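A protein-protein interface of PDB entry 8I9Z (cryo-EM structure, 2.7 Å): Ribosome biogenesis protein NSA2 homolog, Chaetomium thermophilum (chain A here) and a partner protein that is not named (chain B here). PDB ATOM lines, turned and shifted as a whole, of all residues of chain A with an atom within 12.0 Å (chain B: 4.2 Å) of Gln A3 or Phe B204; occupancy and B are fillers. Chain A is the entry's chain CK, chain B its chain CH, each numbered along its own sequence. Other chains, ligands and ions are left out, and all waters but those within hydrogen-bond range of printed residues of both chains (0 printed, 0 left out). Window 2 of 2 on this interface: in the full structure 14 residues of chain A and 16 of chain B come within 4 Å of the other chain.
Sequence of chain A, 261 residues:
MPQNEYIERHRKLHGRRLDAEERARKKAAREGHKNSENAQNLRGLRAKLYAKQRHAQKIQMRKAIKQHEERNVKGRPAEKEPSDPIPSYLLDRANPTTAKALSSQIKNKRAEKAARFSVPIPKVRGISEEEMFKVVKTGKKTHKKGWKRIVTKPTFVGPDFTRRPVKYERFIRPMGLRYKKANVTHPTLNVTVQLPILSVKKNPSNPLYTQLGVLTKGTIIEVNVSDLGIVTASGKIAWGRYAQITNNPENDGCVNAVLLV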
ATOM      1  N   PRO A   2     -24.738  14.756  14.054  1.00  0.00           N
ATOM      2  CA  PRO A   2     -24.861  16.002  13.305  1.00  0.00           C
ATOM      3  C   PRO A   2     -26.171  16.062  12.533  1.00  0.00           C
ATOM      4  O   PRO A   2     -26.627  15.061  11.989  1.00  0.00           O
ATOM      5  CB  PRO A   2     -23.650  15.968  12.380  1.00  0.00           C
ATOM      6  CG  PRO A   2     -23.252  14.529  12.289  1.00  0.00           C
ATOM      7  CD  PRO A   2     -24.031  13.733  13.278  1.00  0.00           C
ATOM      8  N   GLN A   3     -26.784  17.238  12.500  1.00  0.00           N
ATOM      9  CA  GLN A   3     -28.166  17.297  12.055  1.00  0.00           C
ATOM     10  C   GLN A   3     -28.304  17.763  10.615  1.00  0.00           C
ATOM     11  O   GLN A   3     -28.631  16.964   9.738  1.00  0.00           O
ATOM     12  CB  GLN A   3     -28.946  18.206  13.001  1.00  0.00           C
ATOM     13  CG  GLN A   3     -28.073  19.267  13.641  1.00  0.00           C
ATOM     14  CD  GLN A   3     -28.703  19.885  14.857  1.00  0.00           C
ATOM     15  OE1 GLN A   3     -29.882  19.684  15.130  1.00  0.00           O
ATOM     16  NE2 GLN A   3     -27.914  20.633  15.611  1.00  0.00           N
ATOM     17  N   ASN A   4     -27.961  19.007  10.339  1.00  0.00           N
ATOM     18  CA  ASN A   4     -28.156  19.577   9.016  1.00  0.00           C
ATOM     19  C   ASN A   4     -26.881  19.325   8.216  1.00  0.00           C
ATOM     20  O   ASN A   4     -26.083  18.471   8.601  1.00  0.00           O
ATOM     21  CB  ASN A   4     -28.573  21.040   9.145  1.00  0.00           C
ATOM     22  CG  ASN A   4     -29.997  21.181   9.629  1.00  0.00           C
ATOM     23  OD1 ASN A   4     -30.938  20.818   8.929  1.00  0.00           O
ATOM     24  ND2 ASN A   4     -30.164  21.683  10.841  1.00  0.00           N
ATOM     25  N   GLU A   5     -26.648  20.059   7.129  1.00  0.00           N
ATOM     26  CA  GLU A   5     -25.661  19.670   6.119  1.00  0.00           C
ATOM     27  C   GLU A   5     -24.252  19.760   6.705  1.00  0.00           C
ATOM     28  O   GLU A   5     -23.544  20.759   6.571  1.00  0.00           O
ATOM     29  CB  GLU A   5     -25.804  20.563   4.895  1.00  0.00           C
ATOM     30  CG  GLU A   5     -27.232  20.787   4.456  1.00  0.00           C
ATOM     31  CD  GLU A   5     -27.328  21.285   3.032  1.00  0.00           C
ATOM     32  OE1 GLU A   5     -26.501  22.136   2.640  1.00  0.00           O
ATOM     33  OE2 GLU A   5     -28.232  20.827   2.301  1.00  0.00           O
ATOM     34  N   TYR A   6     -23.843  18.668   7.373  1.00  0.00           N
ATOM     35  CA  TYR A   6     -22.646  18.698   8.208  1.00  0.00           C
ATOM     36  C   TYR A   6     -21.360  18.703   7.394  1.00  0.00           C
ATOM     37  O   TYR A   6     -20.389  19.350   7.794  1.00  0.00           O
ATOM     38  CB  TYR A   6     -22.582  17.512   9.180  1.00  0.00           C
ATOM     39  CG  TYR A   6     -23.220  16.191   8.780  1.00  0.00           C
ATOM     40  CD1 TYR A   6     -24.563  15.940   8.978  1.00  0.00           C
ATOM     41  CD2 TYR A   6     -22.442  15.162   8.268  1.00  0.00           C
ATOM     42  CE1 TYR A   6     -25.127  14.736   8.644  1.00  0.00           C
ATOM     43  CE2 TYR A   6     -22.998  13.947   7.928  1.00  0.00           C
ATOM     44  CZ  TYR A   6     -24.344  13.741   8.119  1.00  0.00           C
ATOM     45  OH  TYR A   6     -24.912  12.536   7.781  1.00  0.00           O
ATOM     46  N   ILE A   7     -21.319  17.968   6.281  1.00  0.00           N
ATOM     47  CA  ILE A   7     -20.103  17.900   5.475  1.00  0.00           C
ATOM     48  C   ILE A   7     -19.819  19.246   4.821  1.00  0.00           C
ATOM     49  O   ILE A   7     -18.662  19.674   4.727  1.00  0.00           O
ATOM     50  CB  ILE A   7     -20.215  16.762   4.443  1.00  0.00           C
ATOM     51  CG1 ILE A   7     -20.370  15.418   5.152  1.00  0.00           C
ATOM     52  CG2 ILE A   7     -19.006  16.723   3.524  1.00  0.00           C
ATOM     53  CD1 ILE A   7     -19.159  15.000   5.939  1.00  0.00           C
ATOM     54  N   GLU A   8     -20.866  19.943   4.377  1.00  0.00           N
ATOM     55  CA  GLU A   8     -20.686  21.296   3.859  1.00  0.00           C
ATOM     56  C   GLU A   8     -20.232  22.246   4.958  1.00  0.00           C
ATOM     57  O   GLU A   8     -19.478  23.191   4.701  1.00  0.00           O
ATOM     58  CB  GLU A   8     -21.979  21.791   3.218  1.00  0.00           C
ATOM     59  CG  GLU A   8     -22.395  21.012   1.991  1.00  0.00           C
ATOM     60  CD  GLU A   8     -21.452  21.218   0.824  1.00  0.00           C
ATOM     61  OE1 GLU A   8     -20.922  22.340   0.675  1.00  0.00           O
ATOM     62  OE2 GLU A   8     -21.239  20.259   0.053  1.00  0.00           O
ATOM     63  N   ARG A   9     -20.686  22.014   6.190  1.00  0.00           N
ATOM     64  CA  ARG A   9     -20.200  22.794   7.322  1.00  0.00           C
ATOM     65  C   ARG A   9     -18.749  22.456   7.636  1.00  0.00           C
ATOM     66  O   ARG A   9     -17.965  23.334   8.014  1.00  0.00           O
ATOM     67  CB  ARG A   9     -21.096  22.549   8.533  1.00  0.00           C
ATOM     68  CG  ARG A   9     -20.690  23.288   9.785  1.00  0.00           C
ATOM     69  CD  ARG A   9     -21.609  24.451  10.062  1.00  0.00           C
ATOM     70  NE  ARG A   9     -21.006  25.392  10.995  1.00  0.00           N
ATOM     71  CZ  ARG A   9     -20.937  26.700  10.802  1.00  0.00           C
ATOM     72  NH1 ARG A   9     -21.416  27.262   9.705  1.00  0.00           N
ATOM     73  NH2 ARG A   9     -20.371  27.464  11.731  1.00  0.00           N
ATOM     74  N   HIS A  10     -18.374  21.184   7.485  1.00  0.00           N
ATOM     75  CA  HIS A  10     -16.981  20.783   7.646  1.00  0.00           C
ATOM     76  C   HIS A  10     -16.108  21.365   6.542  1.00  0.00           C
ATOM     77  O   HIS A  10     -14.919  21.626   6.751  1.00  0.00           O
ATOM     78  CB  HIS A  10     -16.888  19.258   7.658  1.00  0.00           C
ATOM     79  CG  HIS A  10     -15.620  18.727   8.246  1.00  0.00           C
ATOM     80  ND1 HIS A  10     -15.402  18.654   9.604  1.00  0.00           N
ATOM     81  CD2 HIS A  10     -14.504  18.237   7.660  1.00  0.00           C
ATOM     82  CE1 HIS A  10     -14.206  18.142   9.829  1.00  0.00           C
ATOM     83  NE2 HIS A  10     -13.640  17.882   8.666  1.00  0.00           N
ATOM     84  N   LYS A  12     -16.553  24.348   5.118  1.00  0.00           N
ATOM     85  CA  LYS A  12     -16.352  25.772   5.342  1.00  0.00           C
ATOM     86  C   LYS A  12     -15.429  26.028   6.521  1.00  0.00           C
ATOM     87  O   LYS A  12     -14.753  27.062   6.572  1.00  0.00           O
ATOM     88  CB  LYS A  12     -17.698  26.457   5.559  1.00  0.00           C
ATOM     89  CG  LYS A  12     -18.561  26.536   4.317  1.00  0.00           C
ATOM     90  CD  LYS A  12     -19.980  26.954   4.663  1.00  0.00           C
ATOM     91  CE  LYS A  12     -20.027  28.372   5.208  1.00  0.00           C
ATOM     92  NZ  LYS A  12     -19.665  29.377   4.172  1.00  0.00           N
ATOM     93  N   LEU A  13     -15.391  25.112   7.483  1.00  0.00           N
ATOM     94  CA  LEU A  13     -14.627  25.355   8.699  1.00  0.00           C
ATOM     95  C   LEU A  13     -13.208  24.806   8.638  1.00  0.00           C
ATOM     96  O   LEU A  13     -12.297  25.404   9.218  1.00  0.00           O
ATOM     97  CB  LEU A  13     -15.355  24.765   9.907  1.00  0.00           C
ATOM     98  CG  LEU A  13     -16.656  25.424  10.351  1.00  0.00           C
ATOM     99  CD1 LEU A  13     -17.140  24.802  11.645  1.00  0.00           C
ATOM    100  CD2 LEU A  13     -16.471  26.913  10.521  1.00  0.00           C
ATOM    101  N   ARG B 158     -30.468  13.235   7.287  1.00  0.00           N
ATOM    102  CA  ARG B 158     -29.909  14.420   7.913  1.00  0.00           C
ATOM    103  C   ARG B 158     -30.981  15.278   8.566  1.00  0.00           C
ATOM    104  O   ARG B 158     -30.969  16.504   8.415  1.00  0.00           O
ATOM    105  CB  ARG B 158     -29.124  15.229   6.883  1.00  0.00           C
ATOM    106  CG  ARG B 158     -27.963  14.469   6.280  1.00  0.00           C
ATOM    107  CD  ARG B 158     -27.042  15.383   5.508  1.00  0.00           C
ATOM    108  NE  ARG B 158     -27.778  16.359   4.715  1.00  0.00           N
ATOM    109  CZ  ARG B 158     -28.246  16.138   3.496  1.00  0.00           C
ATOM    110  NH1 ARG B 158     -28.102  14.966   2.901  1.00  0.00           N
ATOM    111  NH2 ARG B 158     -28.880  17.116   2.857  1.00  0.00           N
ATOM    112  N   LEU B 159     -31.953  14.662   9.189  1.00  0.00           N
ATOM    113  CA  LEU B 159     -32.953  15.409   9.928  1.00  0.00           C
ATOM    114  C   LEU B 159     -32.736  15.208  11.425  1.00  0.00           C
ATOM    115  O   LEU B 159     -32.530  14.078  11.874  1.00  0.00           O
ATOM    116  CB  LEU B 159     -34.355  14.958   9.537  1.00  0.00           C
ATOM    117  CG  LEU B 159     -35.426  16.043   9.469  1.00  0.00           C
ATOM    118  CD1 LEU B 159     -34.973  17.169   8.564  1.00  0.00           C
ATOM    119  CD2 LEU B 159     -36.734  15.458   8.980  1.00  0.00           C
ATOM    120  N   PRO B 160     -32.754  16.279  12.206  1.00  0.00           N
ATOM    121  CA  PRO B 160     -32.520  16.152  13.645  1.00  0.00           C
ATOM    122  C   PRO B 160     -33.652  15.436  14.357  1.00  0.00           C
ATOM    123  O   PRO B 160     -34.804  15.423  13.920  1.00  0.00           O
ATOM    124  CB  PRO B 160     -32.408  17.603  14.110  1.00  0.00           C
ATOM    125  CG  PRO B 160     -33.156  18.373  13.106  1.00  0.00           C
ATOM    126  CD  PRO B 160     -32.940  17.681  11.803  1.00  0.00           C
ATOM    127  N   ASP B 190     -23.856  23.030  17.006  1.00  0.00           N
ATOM    128  CA  ASP B 190     -23.220  23.863  15.987  1.00  0.00           C
ATOM    129  C   ASP B 190     -24.300  24.542  15.158  1.00  0.00           C
ATOM    130  O   ASP B 190     -24.770  23.998  14.157  1.00  0.00           O
ATOM    131  CB  ASP B 190     -22.293  23.029  15.113  1.00  0.00           C
ATOM    132  CG  ASP B 190     -21.123  23.831  14.578  1.00  0.00           C
ATOM    133  OD1 ASP B 190     -21.303  25.035  14.300  1.00  0.00           O
ATOM    134  OD2 ASP B 190     -20.023  23.257  14.433  1.00  0.00           O
ATOM    135  N   THR B 191     -24.698  25.741  15.576  1.00  0.00           N
ATOM    136  CA  THR B 191     -25.679  26.550  14.856  1.00  0.00           C
ATOM    137  C   THR B 191     -24.958  27.767  14.297  1.00  0.00           C
ATOM    138  O   THR B 191     -24.332  28.520  15.064  1.00  0.00           O
ATOM    139  CB  THR B 191     -26.834  26.967  15.756  1.00  0.00           C
ATOM    140  OG1 THR B 191     -27.237  25.857  16.565  1.00  0.00           O
ATOM    141  CG2 THR B 191     -28.015  27.425  14.921  1.00  0.00           C
ATOM    142  N   PRO B 192     -24.982  27.968  12.974  1.00  0.00           N
ATOM    143  CA  PRO B 192     -24.288  29.118  12.375  1.00  0.00           C
ATOM    144  C   PRO B 192     -24.760  30.472  12.876  1.00  0.00           C
ATOM    145  O   PRO B 192     -25.961  30.756  12.882  1.00  0.00           O
ATOM    146  CB  PRO B 192     -24.591  28.968  10.881  1.00  0.00           C
ATOM    147  CG  PRO B 192     -24.957  27.554  10.675  1.00  0.00           C
ATOM    148  CD  PRO B 192     -25.282  26.919  11.987  1.00  0.00           C
ATOM    149  N   THR B 200     -30.058  30.630   9.661  1.00  0.00           N
ATOM    150  CA  THR B 200     -30.636  29.356  10.060  1.00  0.00           C
ATOM    151  C   THR B 200     -31.682  28.960   9.030  1.00  0.00           C
ATOM    152  O   THR B 200     -32.783  29.517   9.002  1.00  0.00           O
ATOM    153  CB  THR B 200     -31.240  29.458  11.456  1.00  0.00           C
ATOM    154  OG1 THR B 200     -30.441  30.336  12.258  1.00  0.00           O
ATOM    155  CG2 THR B 200     -31.285  28.089  12.106  1.00  0.00           C
ATOM    156  N   SER B 202     -32.926  25.852   8.738  1.00  0.00           N
ATOM    157  CA  SER B 202     -33.667  24.681   9.169  1.00  0.00           C
ATOM    158  C   SER B 202     -33.788  24.697  10.685  1.00  0.00           C
ATOM    159  O   SER B 202     -33.536  25.713  11.340  1.00  0.00           O
ATOM    160  CB  SER B 202     -32.993  23.392   8.689  1.00  0.00           C
ATOM    161  OG  SER B 202     -32.713  23.434   7.301  1.00  0.00           O
ATOM    162  N   LEU B 203     -34.180  23.558  11.239  1.00  0.00           N
ATOM    163  CA  LEU B 203     -34.374  23.402  12.672  1.00  0.00           C
ATOM    164  C   LEU B 203     -33.136  22.751  13.270  1.00  0.00           C
ATOM    165  O   LEU B 203     -32.789  21.622  12.909  1.00  0.00           O
ATOM    166  CB  LEU B 203     -35.616  22.558  12.957  1.00  0.00           C
ATOM    167  CG  LEU B 203     -36.836  23.241  13.572  1.00  0.00           C
ATOM    168  CD1 LEU B 203     -37.262  24.438  12.755  1.00  0.00           C
ATOM    169  CD2 LEU B 203     -37.978  22.254  13.698  1.00  0.00           C
ATOM    170  N   PHE B 204     -32.469  23.463  14.168  1.00  0.00           N
ATOM    171  CA  PHE B 204     -31.309  22.952  14.880  1.00  0.00           C
ATOM    172  C   PHE B 204     -31.689  22.635  16.321  1.00  0.00           C
ATOM    173  O   PHE B 204     -32.442  23.376  16.955  1.00  0.00           O
ATOM    174  CB  PHE B 204     -30.165  23.964  14.863  1.00  0.00           C
ATOM    175  CG  PHE B 204     -29.393  23.997  13.578  1.00  0.00           C
ATOM    176  CD1 PHE B 204     -29.877  24.692  12.487  1.00  0.00           C
ATOM    177  CD2 PHE B 204     -28.172  23.359  13.468  1.00  0.00           C
ATOM    178  CE1 PHE B 204     -29.165  24.738  11.309  1.00  0.00           C
ATOM    179  CE2 PHE B 204     -27.460  23.400  12.291  1.00  0.00           C
ATOM    180  CZ  PHE B 204     -27.955  24.091  11.213  1.00  0.00           C
ATOM    181  N   VAL B 205     -31.162  21.528  16.838  1.00  0.00           N
ATOM    182  CA  VAL B 205     -31.503  21.040  18.171  1.00  0.00           C
ATOM    183  C   VAL B 205     -30.255  21.035  19.039  1.00  0.00           C
ATOM    184  O   VAL B 205     -29.185  20.604  18.596  1.00  0.00           O
ATOM    185  CB  VAL B 205     -32.129  19.636  18.122  1.00  0.00           C
ATOM    186  CG1 VAL B 205     -32.706  19.264  19.471  1.00  0.00           C
ATOM    187  CG2 VAL B 205     -33.192  19.582  17.063  1.00  0.00           C
ATOM    188  N   VAL B 217     -33.323  22.229  23.393  1.00  0.00           N
ATOM    189  CA  VAL B 217     -33.398  23.595  22.887  1.00  0.00           C
ATOM    190  C   VAL B 217     -33.469  23.520  21.370  1.00  0.00           C
ATOM    191  O   VAL B 217     -32.552  22.993  20.728  1.00  0.00           O
ATOM    192  CB  VAL B 217     -32.198  24.443  23.335  1.00  0.00           C
ATOM    193  CG1 VAL B 217     -32.400  25.889  22.938  1.00  0.00           C
ATOM    194  CG2 VAL B 217     -31.994  24.333  24.830  1.00  0.00           C
ATOM    195  N   ILE B 218     -34.546  24.045  20.798  1.00  0.00           N
ATOM    196  CA  ILE B 218     -34.759  24.027  19.355  1.00  0.00           C
ATOM    197  C   ILE B 218     -34.461  25.427  18.837  1.00  0.00           C
ATOM    198  O   ILE B 218     -35.030  26.413  19.308  1.00  0.00           O
ATOM    199  CB  ILE B 218     -36.178  23.589  18.985  1.00  0.00           C
ATOM    200  CG1 ILE B 218     -36.638  22.425  19.855  1.00  0.00           C
ATOM    201  CG2 ILE B 218     -36.261  23.239  17.513  1.00  0.00           C
ATOM    202  CD1 ILE B 218     -35.928  21.135  19.577  1.00  0.00           C
ATOM    203  N   ASP B 219     -33.560  25.518  17.865  1.00  0.00           N
ATOM    204  CA  ASP B 219     -33.319  26.780  17.183  1.00  0.00           C
ATOM    205  C   ASP B 219     -34.103  26.815  15.879  1.00  0.00           C
ATOM    206  O   ASP B 219     -33.960  25.927  15.034  1.00  0.00           O
ATOM    207  CB  ASP B 219     -31.832  26.972  16.921  1.00  0.00           C
ATOM    208  CG  ASP B 219     -31.496  28.393  16.543  1.00  0.00           C
ATOM    209  OD1 ASP B 219     -31.583  29.277  17.419  1.00  0.00           O
ATOM    210  OD2 ASP B 219     -31.144  28.631  15.372  1.00  0.00           O
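N of Val B205 lies within hydrogen-bond range of OE1 of Gln A3 (2.8 Å).
The backbone carbonyl oxygen (O) of Leu B203 is in hydrogen-bond range of the side-chain amide nitrogen (ND2) of Asn A4, 3.3 Å away.
The side-chain carboxylate (OD1) of Asp B190 lies within salt-bridge range of the guanidinium group (NE) of Arg A9 (3.3 Å).
OE2 of Glu A5 is in salt-bridge range of NH2 of Arg B158, at 3.8 Å.
The backbone carbonyl oxygen of Arg B158 sits close to the backbone carbonyl oxygen of Gln A3, at 2.7 Å.
O of Phe B204 sits at hydrogen-bond distance from N of Asp B219 (2.6 Å).
OE1 of Gln A3 touches CB of Pro B160, 3.4 Å away.
Phe B204 touches Gln A3 (CD2 to NE2, 3.5 Å).
Asn A4 touches Ser B202 (OD1 to CB, 3.3 Å).
Asn A4 touches Phe B204.
Tyr A6 touches Arg B158.
Pro B192 touches Arg A9.
Gln A3 touches just these residues of chain B: Arg B158, Pro B160, Phe B204 and Val B205.
Phe B204 touches two residues of chain A.
Of the printed residues of chain A, Arg B158 touches Gln A3 (2.7 Å), Glu A5 (3.8 Å) and Tyr A6 (3.7 Å).
Pro B160 touches one residue of chain A.
Of chain A, only Arg A9 (3.3 Å) comes within 4 Å of Asp B190.
No residue of chain A comes within 4 Å of Thr B191.
Of chain A, only Asn A4 comes within 4 Å of Ser B202.
Of chain A, only Asn A4 (3.3 Å) comes within 4 Å of Leu B203.
No residue of chain A comes within 4 Å of Val B217.
No residue of chain A comes within 4 Å of Ile B218.
No residue of chain A comes within 4 Å of Asp B219.
Of the printed residues of chain B, Asn A4 touches Ser B202 (3.3 Å), Leu B203 (3.3 Å) and Phe B204 (3.2 Å).
Of the printed residues of chain B, Arg A9 touches Asp B190 (3.3 Å) and Pro B192 (3.7 Å).
Of the printed residues of chain B, Glu A5 touches Arg B158 (3.8 Å).
Printed residues of chain B within 4 Å of Tyr A6: Arg B158.
The nearest printed residue of chain B that does not touch Asn A4 is Arg B158 (4.2 Å).
Of the 11 printed residues of chain A, 5 touch a printed residue of chain B.
Printed residues of chain A that touch a printed residue of chain B: Gln A3, Asn A4, Glu A5, Tyr A6 and Arg A9.
Along chain A the printed residues that touch a printed residue of chain B span positions 3 to 9.
Among the printed residues, Asp or Glu carboxylates within 4 Å of a Lys or Arg side-chain nitrogen of the other chain: Glu A5 with Arg B158 (3.8 Å) and Arg A9 with Asp B190 (3.3 Å).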
